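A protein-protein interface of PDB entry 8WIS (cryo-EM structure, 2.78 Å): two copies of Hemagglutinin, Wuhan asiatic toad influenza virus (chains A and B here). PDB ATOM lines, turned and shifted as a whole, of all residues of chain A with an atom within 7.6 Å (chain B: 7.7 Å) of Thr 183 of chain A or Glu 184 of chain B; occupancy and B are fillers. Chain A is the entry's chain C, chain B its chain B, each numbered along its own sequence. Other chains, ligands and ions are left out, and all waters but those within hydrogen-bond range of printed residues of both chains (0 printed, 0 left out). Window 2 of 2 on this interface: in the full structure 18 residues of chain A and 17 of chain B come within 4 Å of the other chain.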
ATOM      1  N   GLU A 171     -15.855   9.005  10.958  1.00  0.00           N
ATOM      2  CA  GLU A 171     -16.363   8.295   9.789  1.00  0.00           C
ATOM      3  C   GLU A 171     -16.788   9.257   8.691  1.00  0.00           C
ATOM      4  O   GLU A 171     -16.623   8.956   7.502  1.00  0.00           O
ATOM      5  CB  GLU A 171     -17.532   7.398  10.191  1.00  0.00           C
ATOM      6  CG  GLU A 171     -17.117   6.120  10.895  1.00  0.00           C
ATOM      7  CD  GLU A 171     -18.219   5.081  10.918  1.00  0.00           C
ATOM      8  OE1 GLU A 171     -19.388   5.446  10.677  1.00  0.00           O
ATOM      9  OE2 GLU A 171     -17.915   3.898  11.179  1.00  0.00           O
ATOM     10  N   TYR A 174     -13.744  10.340   6.664  1.00  0.00           N
ATOM     11  CA  TYR A 174     -13.250   9.226   5.862  1.00  0.00           C
ATOM     12  C   TYR A 174     -14.132   8.996   4.643  1.00  0.00           C
ATOM     13  O   TYR A 174     -13.627   8.793   3.532  1.00  0.00           O
ATOM     14  CB  TYR A 174     -13.173   7.966   6.725  1.00  0.00           C
ATOM     15  CG  TYR A 174     -12.727   6.714   6.003  1.00  0.00           C
ATOM     16  CD1 TYR A 174     -11.391   6.346   5.978  1.00  0.00           C
ATOM     17  CD2 TYR A 174     -13.643   5.887   5.369  1.00  0.00           C
ATOM     18  CE1 TYR A 174     -10.980   5.202   5.329  1.00  0.00           C
ATOM     19  CE2 TYR A 174     -13.240   4.742   4.718  1.00  0.00           C
ATOM     20  CZ  TYR A 174     -11.908   4.404   4.701  1.00  0.00           C
ATOM     21  OH  TYR A 174     -11.502   3.262   4.054  1.00  0.00           O
ATOM     22  N   ARG A 180     -15.398   5.712  -0.341  1.00  0.00           N
ATOM     23  CA  ARG A 180     -15.617   4.279  -0.242  1.00  0.00           C
ATOM     24  C   ARG A 180     -16.499   3.962   0.959  1.00  0.00           C
ATOM     25  O   ARG A 180     -16.657   4.778   1.870  1.00  0.00           O
ATOM     26  CB  ARG A 180     -14.288   3.534  -0.107  1.00  0.00           C
ATOM     27  CG  ARG A 180     -13.396   3.609  -1.328  1.00  0.00           C
ATOM     28  CD  ARG A 180     -12.188   2.705  -1.167  1.00  0.00           C
ATOM     29  NE  ARG A 180     -11.128   3.029  -2.112  1.00  0.00           N
ATOM     30  CZ  ARG A 180     -10.841   2.307  -3.186  1.00  0.00           C
ATOM     31  NH1 ARG A 180     -11.523   1.215  -3.485  1.00  0.00           N
ATOM     32  NH2 ARG A 180      -9.847   2.692  -3.980  1.00  0.00           N
ATOM     33  N   ASN A 181     -17.077   2.766   0.948  1.00  0.00           N
ATOM     34  CA  ASN A 181     -17.841   2.302   2.094  1.00  0.00           C
ATOM     35  C   ASN A 181     -16.906   1.935   3.240  1.00  0.00           C
ATOM     36  O   ASN A 181     -15.759   1.533   3.032  1.00  0.00           O
ATOM     37  CB  ASN A 181     -18.701   1.101   1.712  1.00  0.00           C
ATOM     38  CG  ASN A 181     -20.133   1.485   1.412  1.00  0.00           C
ATOM     39  OD1 ASN A 181     -20.710   2.342   2.079  1.00  0.00           O
ATOM     40  ND2 ASN A 181     -20.714   0.852   0.402  1.00  0.00           N
ATOM     41  N   VAL A 182     -17.410   2.081   4.466  1.00  0.00           N
ATOM     42  CA  VAL A 182     -16.584   1.810   5.639  1.00  0.00           C
ATOM     43  C   VAL A 182     -16.239   0.328   5.726  1.00  0.00           C
ATOM     44  O   VAL A 182     -15.193  -0.047   6.269  1.00  0.00           O
ATOM     45  CB  VAL A 182     -17.286   2.310   6.914  1.00  0.00           C
ATOM     46  CG1 VAL A 182     -17.456   3.815   6.862  1.00  0.00           C
ATOM     47  CG2 VAL A 182     -18.635   1.634   7.076  1.00  0.00           C
ATOM     48  N   THR A 183     -17.103  -0.536   5.203  1.00  0.00           N
ATOM     49  CA  THR A 183     -16.846  -1.976   5.196  1.00  0.00           C
ATOM     50  C   THR A 183     -16.097  -2.400   3.938  1.00  0.00           C
ATOM     51  O   THR A 183     -16.503  -3.313   3.223  1.00  0.00           O
ATOM     52  CB  THR A 183     -18.156  -2.741   5.331  1.00  0.00           C
ATOM     53  OG1 THR A 183     -18.979  -2.484   4.187  1.00  0.00           O
ATOM     54  CG2 THR A 183     -18.895  -2.309   6.586  1.00  0.00           C
ATOM     55  N   GLU A 184     -14.982  -1.729   3.664  1.00  0.00           N
ATOM     56  CA  GLU A 184     -14.170  -2.009   2.491  1.00  0.00           C
ATOM     57  C   GLU A 184     -12.704  -1.836   2.843  1.00  0.00           C
ATOM     58  O   GLU A 184     -12.331  -0.877   3.524  1.00  0.00           O
ATOM     59  CB  GLU A 184     -14.529  -1.088   1.322  1.00  0.00           C
ATOM     60  CG  GLU A 184     -15.711  -1.549   0.501  1.00  0.00           C
ATOM     61  CD  GLU A 184     -15.688  -0.982  -0.900  1.00  0.00           C
ATOM     62  OE1 GLU A 184     -14.638  -0.442  -1.303  1.00  0.00           O
ATOM     63  OE2 GLU A 184     -16.720  -1.070  -1.596  1.00  0.00           O
ATOM     64  N   ARG A 185     -11.876  -2.762   2.372  1.00  0.00           N
ATOM     65  CA  ARG A 185     -10.432  -2.686   2.541  1.00  0.00           C
ATOM     66  C   ARG A 185      -9.808  -2.430   1.177  1.00  0.00           C
ATOM     67  O   ARG A 185     -10.042  -3.191   0.234  1.00  0.00           O
ATOM     68  CB  ARG A 185      -9.884  -3.971   3.159  1.00  0.00           C
ATOM     69  CG  ARG A 185      -8.374  -4.083   3.109  1.00  0.00           C
ATOM     70  CD  ARG A 185      -7.888  -5.376   3.738  1.00  0.00           C
ATOM     71  NE  ARG A 185      -8.341  -5.524   5.114  1.00  0.00           N
ATOM     72  CZ  ARG A 185      -7.723  -6.258   6.028  1.00  0.00           C
ATOM     73  NH1 ARG A 185      -6.619  -6.928   5.745  1.00  0.00           N
ATOM     74  NH2 ARG A 185      -8.224  -6.320   7.258  1.00  0.00           N
ATOM     75  N   SER A 201      -8.748   0.652   5.691  1.00  0.00           N
ATOM     76  CA  SER A 201     -10.171   0.366   5.820  1.00  0.00           C
ATOM     77  C   SER A 201     -10.806   1.480   6.645  1.00  0.00           C
ATOM     78  O   SER A 201     -10.191   2.523   6.888  1.00  0.00           O
ATOM     79  CB  SER A 201     -10.401  -1.011   6.448  1.00  0.00           C
ATOM     80  OG  SER A 201     -10.041  -1.006   7.817  1.00  0.00           O
ATOM     81  N   GLY A 202     -12.044   1.255   7.080  1.00  0.00           N
ATOM     82  CA  GLY A 202     -12.774   2.235   7.847  1.00  0.00           C
ATOM     83  C   GLY A 202     -12.139   2.491   9.197  1.00  0.00           C
ATOM     84  O   GLY A 202     -11.395   1.659   9.724  1.00  0.00           O
ATOM     85  N   LYS A 204     -13.358   2.540  12.248  1.00  0.00           N
ATOM     86  CA  LYS A 204     -13.715   1.500  13.212  1.00  0.00           C
ATOM     87  C   LYS A 204     -13.631   0.113  12.587  1.00  0.00           C
ATOM     88  O   LYS A 204     -14.535  -0.707  12.727  1.00  0.00           O
ATOM     89  CB  LYS A 204     -15.108   1.763  13.769  1.00  0.00           C
ATOM     90  CG  LYS A 204     -15.322   3.177  14.263  1.00  0.00           C
ATOM     91  CD  LYS A 204     -16.767   3.401  14.667  1.00  0.00           C
ATOM     92  CE  LYS A 204     -16.899   4.620  15.558  1.00  0.00           C
ATOM     93  NZ  LYS A 204     -15.719   4.773  16.452  1.00  0.00           N
ATOM     94  N   GLN A 205     -12.516  -0.168  11.918  1.00  0.00           N
ATOM     95  CA  GLN A 205     -12.335  -1.426  11.210  1.00  0.00           C
ATOM     96  C   GLN A 205     -10.849  -1.724  11.104  1.00  0.00           C
ATOM     97  O   GLN A 205     -10.033  -0.809  10.973  1.00  0.00           O
ATOM     98  CB  GLN A 205     -12.951  -1.388   9.805  1.00  0.00           C
ATOM     99  CG  GLN A 205     -14.398  -1.835   9.723  1.00  0.00           C
ATOM    100  CD  GLN A 205     -15.373  -0.696   9.918  1.00  0.00           C
ATOM    101  OE1 GLN A 205     -14.999   0.472   9.857  1.00  0.00           O
ATOM    102  NE2 GLN A 205     -16.634  -1.032  10.158  1.00  0.00           N
ATOM    103  N   SER A 206     -10.509  -3.006  11.162  1.00  0.00           N
ATOM    104  CA  SER A 206      -9.139  -3.420  10.930  1.00  0.00           C
ATOM    105  C   SER A 206      -8.761  -3.158   9.473  1.00  0.00           C
ATOM    106  O   SER A 206      -9.593  -3.297   8.574  1.00  0.00           O
ATOM    107  CB  SER A 206      -8.975  -4.900  11.262  1.00  0.00           C
ATOM    108  OG  SER A 206      -7.641  -5.336  11.080  1.00  0.00           O
ATOM    109  N   GLU A 209      -7.948   0.578  12.851  1.00  0.00           N
ATOM    110  CA  GLU A 209      -8.179   0.774  14.278  1.00  0.00           C
ATOM    111  C   GLU A 209      -6.890   0.640  15.075  1.00  0.00           C
ATOM    112  O   GLU A 209      -6.759   1.242  16.146  1.00  0.00           O
ATOM    113  CB  GLU A 209      -9.220  -0.217  14.794  1.00  0.00           C
ATOM    114  CG  GLU A 209      -8.901  -1.667  14.491  1.00  0.00           C
ATOM    115  CD  GLU A 209     -10.049  -2.595  14.826  1.00  0.00           C
ATOM    116  OE1 GLU A 209     -11.210  -2.140  14.799  1.00  0.00           O
ATOM    117  OE2 GLU A 209      -9.789  -3.781  15.117  1.00  0.00           O
ATOM    118  N   PRO B 146     -16.085  -4.793  19.259  1.00  0.00           N
ATOM    119  CA  PRO B 146     -14.841  -5.569  19.277  1.00  0.00           C
ATOM    120  C   PRO B 146     -13.821  -5.035  20.276  1.00  0.00           C
ATOM    121  O   PRO B 146     -13.123  -5.820  20.915  1.00  0.00           O
ATOM    122  CB  PRO B 146     -14.314  -5.426  17.842  1.00  0.00           C
ATOM    123  CG  PRO B 146     -15.389  -4.719  17.071  1.00  0.00           C
ATOM    124  CD  PRO B 146     -16.172  -3.945  18.063  1.00  0.00           C
ATOM    125  N   TYR B 174     -19.945 -17.086  15.577  1.00  0.00           N
ATOM    126  CA  TYR B 174     -18.936 -16.120  15.160  1.00  0.00           C
ATOM    127  C   TYR B 174     -19.388 -14.696  15.450  1.00  0.00           C
ATOM    128  O   TYR B 174     -18.619 -13.886  15.984  1.00  0.00           O
ATOM    129  CB  TYR B 174     -18.637 -16.301  13.671  1.00  0.00           C
ATOM    130  CG  TYR B 174     -17.699 -15.270  13.085  1.00  0.00           C
ATOM    131  CD1 TYR B 174     -16.331 -15.487  13.057  1.00  0.00           C
ATOM    132  CD2 TYR B 174     -18.185 -14.089  12.542  1.00  0.00           C
ATOM    133  CE1 TYR B 174     -15.473 -14.552  12.519  1.00  0.00           C
ATOM    134  CE2 TYR B 174     -17.335 -13.150  12.005  1.00  0.00           C
ATOM    135  CZ  TYR B 174     -15.980 -13.385  11.995  1.00  0.00           C
ATOM    136  OH  TYR B 174     -15.130 -12.450  11.456  1.00  0.00           O
ATOM    137  N   GLY B 179     -18.476 -10.025  17.365  1.00  0.00           N
ATOM    138  CA  GLY B 179     -19.233  -8.795  17.294  1.00  0.00           C
ATOM    139  C   GLY B 179     -19.085  -8.033  15.999  1.00  0.00           C
ATOM    140  O   GLY B 179     -19.417  -6.843  15.958  1.00  0.00           O
ATOM    141  N   ARG B 180     -18.595  -8.674  14.943  1.00  0.00           N
ATOM    142  CA  ARG B 180     -18.405  -8.046  13.646  1.00  0.00           C
ATOM    143  C   ARG B 180     -19.401  -8.603  12.637  1.00  0.00           C
ATOM    144  O   ARG B 180     -20.059  -9.616  12.883  1.00  0.00           O
ATOM    145  CB  ARG B 180     -16.983  -8.277  13.138  1.00  0.00           C
ATOM    146  CG  ARG B 180     -15.909  -7.551  13.917  1.00  0.00           C
ATOM    147  CD  ARG B 180     -14.587  -7.592  13.177  1.00  0.00           C
ATOM    148  NE  ARG B 180     -13.462  -7.263  14.041  1.00  0.00           N
ATOM    149  CZ  ARG B 180     -12.827  -6.100  14.028  1.00  0.00           C
ATOM    150  NH1 ARG B 180     -13.188  -5.126  13.212  1.00  0.00           N
ATOM    151  NH2 ARG B 180     -11.803  -5.910  14.855  1.00  0.00           N
ATOM    152  N   ASN B 181     -19.507  -7.929  11.495  1.00  0.00           N
ATOM    153  CA  ASN B 181     -20.241  -8.489  10.371  1.00  0.00           C
ATOM    154  C   ASN B 181     -19.439  -9.595   9.696  1.00  0.00           C
ATOM    155  O   ASN B 181     -18.212  -9.659   9.799  1.00  0.00           O
ATOM    156  CB  ASN B 181     -20.596  -7.411   9.348  1.00  0.00           C
ATOM    157  CG  ASN B 181     -21.861  -6.661   9.705  1.00  0.00           C
ATOM    158  OD1 ASN B 181     -22.823  -7.253  10.190  1.00  0.00           O
ATOM    159  ND2 ASN B 181     -21.880  -5.361   9.446  1.00  0.00           N
ATOM    160  N   VAL B 182     -20.158 -10.477   9.000  1.00  0.00           N
ATOM    161  CA  VAL B 182     -19.514 -11.611   8.345  1.00  0.00           C
ATOM    162  C   VAL B 182     -18.665 -11.146   7.166  1.00  0.00           C
ATOM    163  O   VAL B 182     -17.591 -11.699   6.906  1.00  0.00           O
ATOM    164  CB  VAL B 182     -20.567 -12.651   7.922  1.00  0.00           C
ATOM    165  CG1 VAL B 182     -21.259 -13.216   9.146  1.00  0.00           C
ATOM    166  CG2 VAL B 182     -21.592 -12.031   6.989  1.00  0.00           C
ATOM    167  N   THR B 183     -19.123 -10.132   6.439  1.00  0.00           N
ATOM    168  CA  THR B 183     -18.400  -9.640   5.266  1.00  0.00           C
ATOM    169  C   THR B 183     -17.330  -8.626   5.654  1.00  0.00           C
ATOM    170  O   THR B 183     -17.254  -7.528   5.105  1.00  0.00           O
ATOM    171  CB  THR B 183     -19.379  -9.041   4.265  1.00  0.00           C
ATOM    172  OG1 THR B 183     -19.921  -7.827   4.798  1.00  0.00           O
ATOM    173  CG2 THR B 183     -20.511 -10.013   3.985  1.00  0.00           C
ATOM    174  N   GLU B 184     -16.485  -8.999   6.611  1.00  0.00           N
ATOM    175  CA  GLU B 184     -15.415  -8.140   7.089  1.00  0.00           C
ATOM    176  C   GLU B 184     -14.180  -8.984   7.347  1.00  0.00           C
ATOM    177  O   GLU B 184     -14.277 -10.092   7.880  1.00  0.00           O
ATOM    178  CB  GLU B 184     -15.815  -7.403   8.371  1.00  0.00           C
ATOM    179  CG  GLU B 184     -16.605  -6.132   8.140  1.00  0.00           C
ATOM    180  CD  GLU B 184     -16.552  -5.200   9.331  1.00  0.00           C
ATOM    181  OE1 GLU B 184     -15.728  -5.440  10.238  1.00  0.00           O
ATOM    182  OE2 GLU B 184     -17.337  -4.229   9.364  1.00  0.00           O
ATOM    183  N   ARG B 185     -13.022  -8.458   6.969  1.00  0.00           N
ATOM    184  CA  ARG B 185     -11.748  -9.131   7.168  1.00  0.00           C
ATOM    185  C   ARG B 185     -10.936  -8.333   8.177  1.00  0.00           C
ATOM    186  O   ARG B 185     -10.681  -7.143   7.967  1.00  0.00           O
ATOM    187  CB  ARG B 185     -10.996  -9.269   5.846  1.00  0.00           C
ATOM    188  CG  ARG B 185      -9.521  -9.567   5.990  1.00  0.00           C
ATOM    189  CD  ARG B 185      -8.889  -9.817   4.634  1.00  0.00           C
ATOM    190  NE  ARG B 185      -9.540 -10.915   3.930  1.00  0.00           N
ATOM    191  CZ  ARG B 185      -8.974 -11.624   2.964  1.00  0.00           C
ATOM    192  NH1 ARG B 185      -7.747 -11.367   2.545  1.00  0.00           N
ATOM    193  NH2 ARG B 185      -9.657 -12.618   2.405  1.00  0.00           N
ATOM    194  N   TRP B 186     -10.535  -8.982   9.267  1.00  0.00           N
ATOM    195  CA  TRP B 186      -9.785  -8.321  10.323  1.00  0.00           C
ATOM    196  C   TRP B 186      -8.486  -9.067  10.586  1.00  0.00           C
ATOM    197  O   TRP B 186      -8.410 -10.289  10.446  1.00  0.00           O
ATOM    198  CB  TRP B 186     -10.605  -8.210  11.615  1.00  0.00           C
ATOM    199  CG  TRP B 186     -11.283  -9.470  12.043  1.00  0.00           C
ATOM    200  CD1 TRP B 186     -12.377 -10.048  11.473  1.00  0.00           C
ATOM    201  CD2 TRP B 186     -10.927 -10.297  13.155  1.00  0.00           C
ATOM    202  NE1 TRP B 186     -12.716 -11.191  12.151  1.00  0.00           N
ATOM    203  CE2 TRP B 186     -11.841 -11.365  13.189  1.00  0.00           C
ATOM    204  CE3 TRP B 186      -9.919 -10.241  14.120  1.00  0.00           C
ATOM    205  CZ2 TRP B 186     -11.777 -12.367  14.150  1.00  0.00           C
ATOM    206  CZ3 TRP B 186      -9.858 -11.236  15.072  1.00  0.00           C
ATOM    207  CH2 TRP B 186     -10.781 -12.285  15.081  1.00  0.00           C
ATOM    208  N   ASP B 187      -7.463  -8.317  10.980  1.00  0.00           N
ATOM    209  CA  ASP B 187      -6.112  -8.839  11.094  1.00  0.00           C
ATOM    210  C   ASP B 187      -5.633  -8.813  12.539  1.00  0.00           C
ATOM    211  O   ASP B 187      -6.040  -7.963  13.336  1.00  0.00           O
ATOM    212  CB  ASP B 187      -5.143  -8.033  10.225  1.00  0.00           C
ATOM    213  CG  ASP B 187      -5.422  -8.189   8.747  1.00  0.00           C
ATOM    214  OD1 ASP B 187      -5.953  -9.247   8.353  1.00  0.00           O
ATOM    215  OD2 ASP B 187      -5.113  -7.256   7.978  1.00  0.00           O
ATOM    216  N   PHE B 200      -8.487 -12.974   9.356  1.00  0.00           N
ATOM    217  CA  PHE B 200      -9.678 -13.760   9.633  1.00  0.00           C
ATOM    218  C   PHE B 200     -10.885 -13.058   9.034  1.00  0.00           C
ATOM    219  O   PHE B 200     -10.880 -11.843   8.817  1.00  0.00           O
ATOM    220  CB  PHE B 200      -9.894 -13.970  11.136  1.00  0.00           C
ATOM    221  CG  PHE B 200      -8.705 -14.539  11.850  1.00  0.00           C
ATOM    222  CD1 PHE B 200      -8.423 -15.890  11.782  1.00  0.00           C
ATOM    223  CD2 PHE B 200      -7.876 -13.725  12.595  1.00  0.00           C
ATOM    224  CE1 PHE B 200      -7.332 -16.415  12.440  1.00  0.00           C
ATOM    225  CE2 PHE B 200      -6.784 -14.244  13.255  1.00  0.00           C
ATOM    226  CZ  PHE B 200      -6.511 -15.591  13.175  1.00  0.00           C
ATOM    227  N   SER B 201     -11.927 -13.838   8.778  1.00  0.00           N
ATOM    228  CA  SER B 201     -13.179 -13.326   8.237  1.00  0.00           C
ATOM    229  C   SER B 201     -14.299 -14.251   8.697  1.00  0.00           C
ATOM    230  O   SER B 201     -14.112 -15.080   9.593  1.00  0.00           O
ATOM    231  CB  SER B 201     -13.113 -13.216   6.713  1.00  0.00           C
ATOM    232  OG  SER B 201     -13.050 -14.500   6.123  1.00  0.00           O
ATOM    233  N   GLY B 202     -15.468 -14.114   8.081  1.00  0.00           N
ATOM    234  CA  GLY B 202     -16.603 -14.935   8.424  1.00  0.00           C
ATOM    235  C   GLY B 202     -16.382 -16.383   8.041  1.00  0.00           C
ATOM    236  O   GLY B 202     -15.451 -16.717   7.303  1.00  0.00           O
ATOM    237  N   GLN B 205     -16.582 -17.237   4.186  1.00  0.00           N
ATOM    238  CA  GLN B 205     -15.825 -16.192   3.514  1.00  0.00           C
ATOM    239  C   GLN B 205     -14.346 -16.529   3.600  1.00  0.00           C
ATOM    240  O   GLN B 205     -13.890 -17.096   4.595  1.00  0.00           O
ATOM    241  CB  GLN B 205     -16.076 -14.812   4.134  1.00  0.00           C
ATOM    242  CG  GLN B 205     -17.293 -14.074   3.604  1.00  0.00           C
ATOM    243  CD  GLN B 205     -18.532 -14.319   4.438  1.00  0.00           C
ATOM    244  OE1 GLN B 205     -18.448 -14.803   5.565  1.00  0.00           O
ATOM    245  NE2 GLN B 205     -19.691 -13.984   3.888  1.00  0.00           N
ATOM    246  N   SER B 206     -13.606 -16.181   2.553  1.00  0.00           N
ATOM    247  CA  SER B 206     -12.166 -16.345   2.584  1.00  0.00           C
ATOM    248  C   SER B 206     -11.558 -15.375   3.597  1.00  0.00           C
ATOM    249  O   SER B 206     -12.051 -14.257   3.765  1.00  0.00           O
ATOM    250  CB  SER B 206     -11.577 -16.100   1.199  1.00  0.00           C
ATOM    251  OG  SER B 206     -10.178 -16.308   1.185  1.00  0.00           O
ATOM    252  N   PRO B 207     -10.480 -15.775   4.289  1.00  0.00           N
ATOM    253  CA  PRO B 207      -9.757 -17.041   4.182  1.00  0.00           C
ATOM    254  C   PRO B 207     -10.071 -18.044   5.284  1.00  0.00           C
ATOM    255  O   PRO B 207      -9.195 -18.830   5.632  1.00  0.00           O
ATOM    256  CB  PRO B 207      -8.303 -16.596   4.285  1.00  0.00           C
ATOM    257  CG  PRO B 207      -8.358 -15.404   5.212  1.00  0.00           C
ATOM    258  CD  PRO B 207      -9.769 -14.845   5.181  1.00  0.00           C
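The guanidinium group (NH2) of Arg 185 of chain A lies within hydrogen-bond range of the backbone carbonyl oxygen (O) of Arg 185 of chain B (2.7 Å). The backbone NH of Asp 187 of chain B sits at hydrogen-bond distance from the side-chain hydroxyl of Ser 206 of chain A (3.0 Å). The side-chain carboxylate (OD2) of Asp 187 of chain B lies within salt-bridge range of the guanidinium group (NH1) of Arg 185 of chain A (2.7 Å). The side-chain carboxylate (OE2) of Glu 184 of chain B is in hydrogen-bond range of the side-chain amide nitrogen (NE2) of Gln 205 of chain A, 3.4 Å away. The guanidinium group (NH2) of Arg 180 of chain B is in salt-bridge range of the side-chain carboxylate (OE2) of Glu 209 of chain A (2.9 Å).
Among the printed residues, pairs that only touch across the chains: Ser 206 of chain A with Trp 186 of chain B (3.6 Å), Thr 183 of chain A with Glu 184 of chain B (3.7 Å), Arg 185 of chain A with Trp 186 of chain B (3.98 Å) and Ser 206 of chain A with Arg 180 of chain B (3.98 Å).
Of the 17 printed residues of chain B, 5 touch a printed residue of chain A. Printed residues of chain A that touch a printed residue of chain B: Thr 183, Arg 185, Gln 205, Ser 206 and Glu 209. Along chain A the printed residues that touch a printed residue of chain B span positions 183 to 209. Among the printed residues, 9 pairs touch across the chains. Among the printed residues, Asp or Glu carboxylates within 4 Å of a Lys or Arg side-chain nitrogen of the other chain: Arg 185 of chain A with Asp 187 of chain B and Glu 209 of chain A with Arg 180 of chain B.
Printed residues of chain B within 4 Å of Thr 183 of chain A: Glu 184. Of chain A, only Thr 183 (3.7 Å) and Gln 205 (3.4 Å) come within 4 Å of Glu 184 of chain B. Of the printed residues of chain B, Glu 209 of chain A touches Arg 180. Printed residues of chain B within 4 Å of Gln 205 of chain A: Glu 184. Of the printed residues of chain A, Arg 185 of chain B touches Arg 185. Printed residues of chain B within 4 Å of Arg 185 of chain A: Arg 185 (2.7 Å), Trp 186 (3.98 Å) and Asp 187 (2.7 Å). The nearest residue of chain B that does not touch Thr 183 of chain A is Thr 183 of chain B (4.7 Å). The nearest residue of chain A that does not touch Glu 184 of chain B is Lys 204 of chain A (5.5 Å). The nearest printed residue of chain B that does not touch Arg 185 of chain A is Phe 200 of chain B (6.3 Å).
Thr 183 of chain A touches Glu 184 of chain B, but with the chains exchanged Glu 184 of chain A does not touch Thr 183 of chain B (6.4 Å). Arg 185 of chain A touches its own counterpart, Arg 185 of chain B. Gln 205 of chain A touches Glu 184 of chain B, but with the chains exchanged Glu 184 of chain A does not touch Gln 205 of chain B (12.5 Å). Ser 206 of chain A touches Arg 180 of chain B, but with the chains exchanged Arg 180 of chain A does not touch Ser 206 of chain B (17.1 Å). Positions printed for both chains: 174, 180, 181, 182, 183, 184, 185, 201, 202, 205 and 206. Of the 9 pairs that touch across the chains among the printed residues, 1 has its exchanged pair printed and touching as well.
The backbone carbonyl oxygen of Gln 205 of chain A is in hydrogen-bond range of the side-chain hydroxyl of Ser 201 of chain A. NH2 of Arg 185 of chain B lies within hydrogen-bond range of O of Ser 206 of chain B, 3.2 Å away. The side-chain hydroxyl (OH) of Tyr 174 of chain B lies within hydrogen-bond range of the indole nitrogen (NE1) of Trp 186 of chain B (2.8 Å). OE1 of Glu 184 of chain B lies within salt-bridge range of NH1 of Arg 180 of chain B, at 3.9 Å. The backbone NH of Phe 200 of chain B sits at hydrogen-bond distance from the backbone carbonyl oxygen of Trp 186 of chain B, 2.9 Å away. OG of Ser 201 of chain A is in hydrogen-bond range of O of Ser 206 of chain A, 2.5 Å away.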
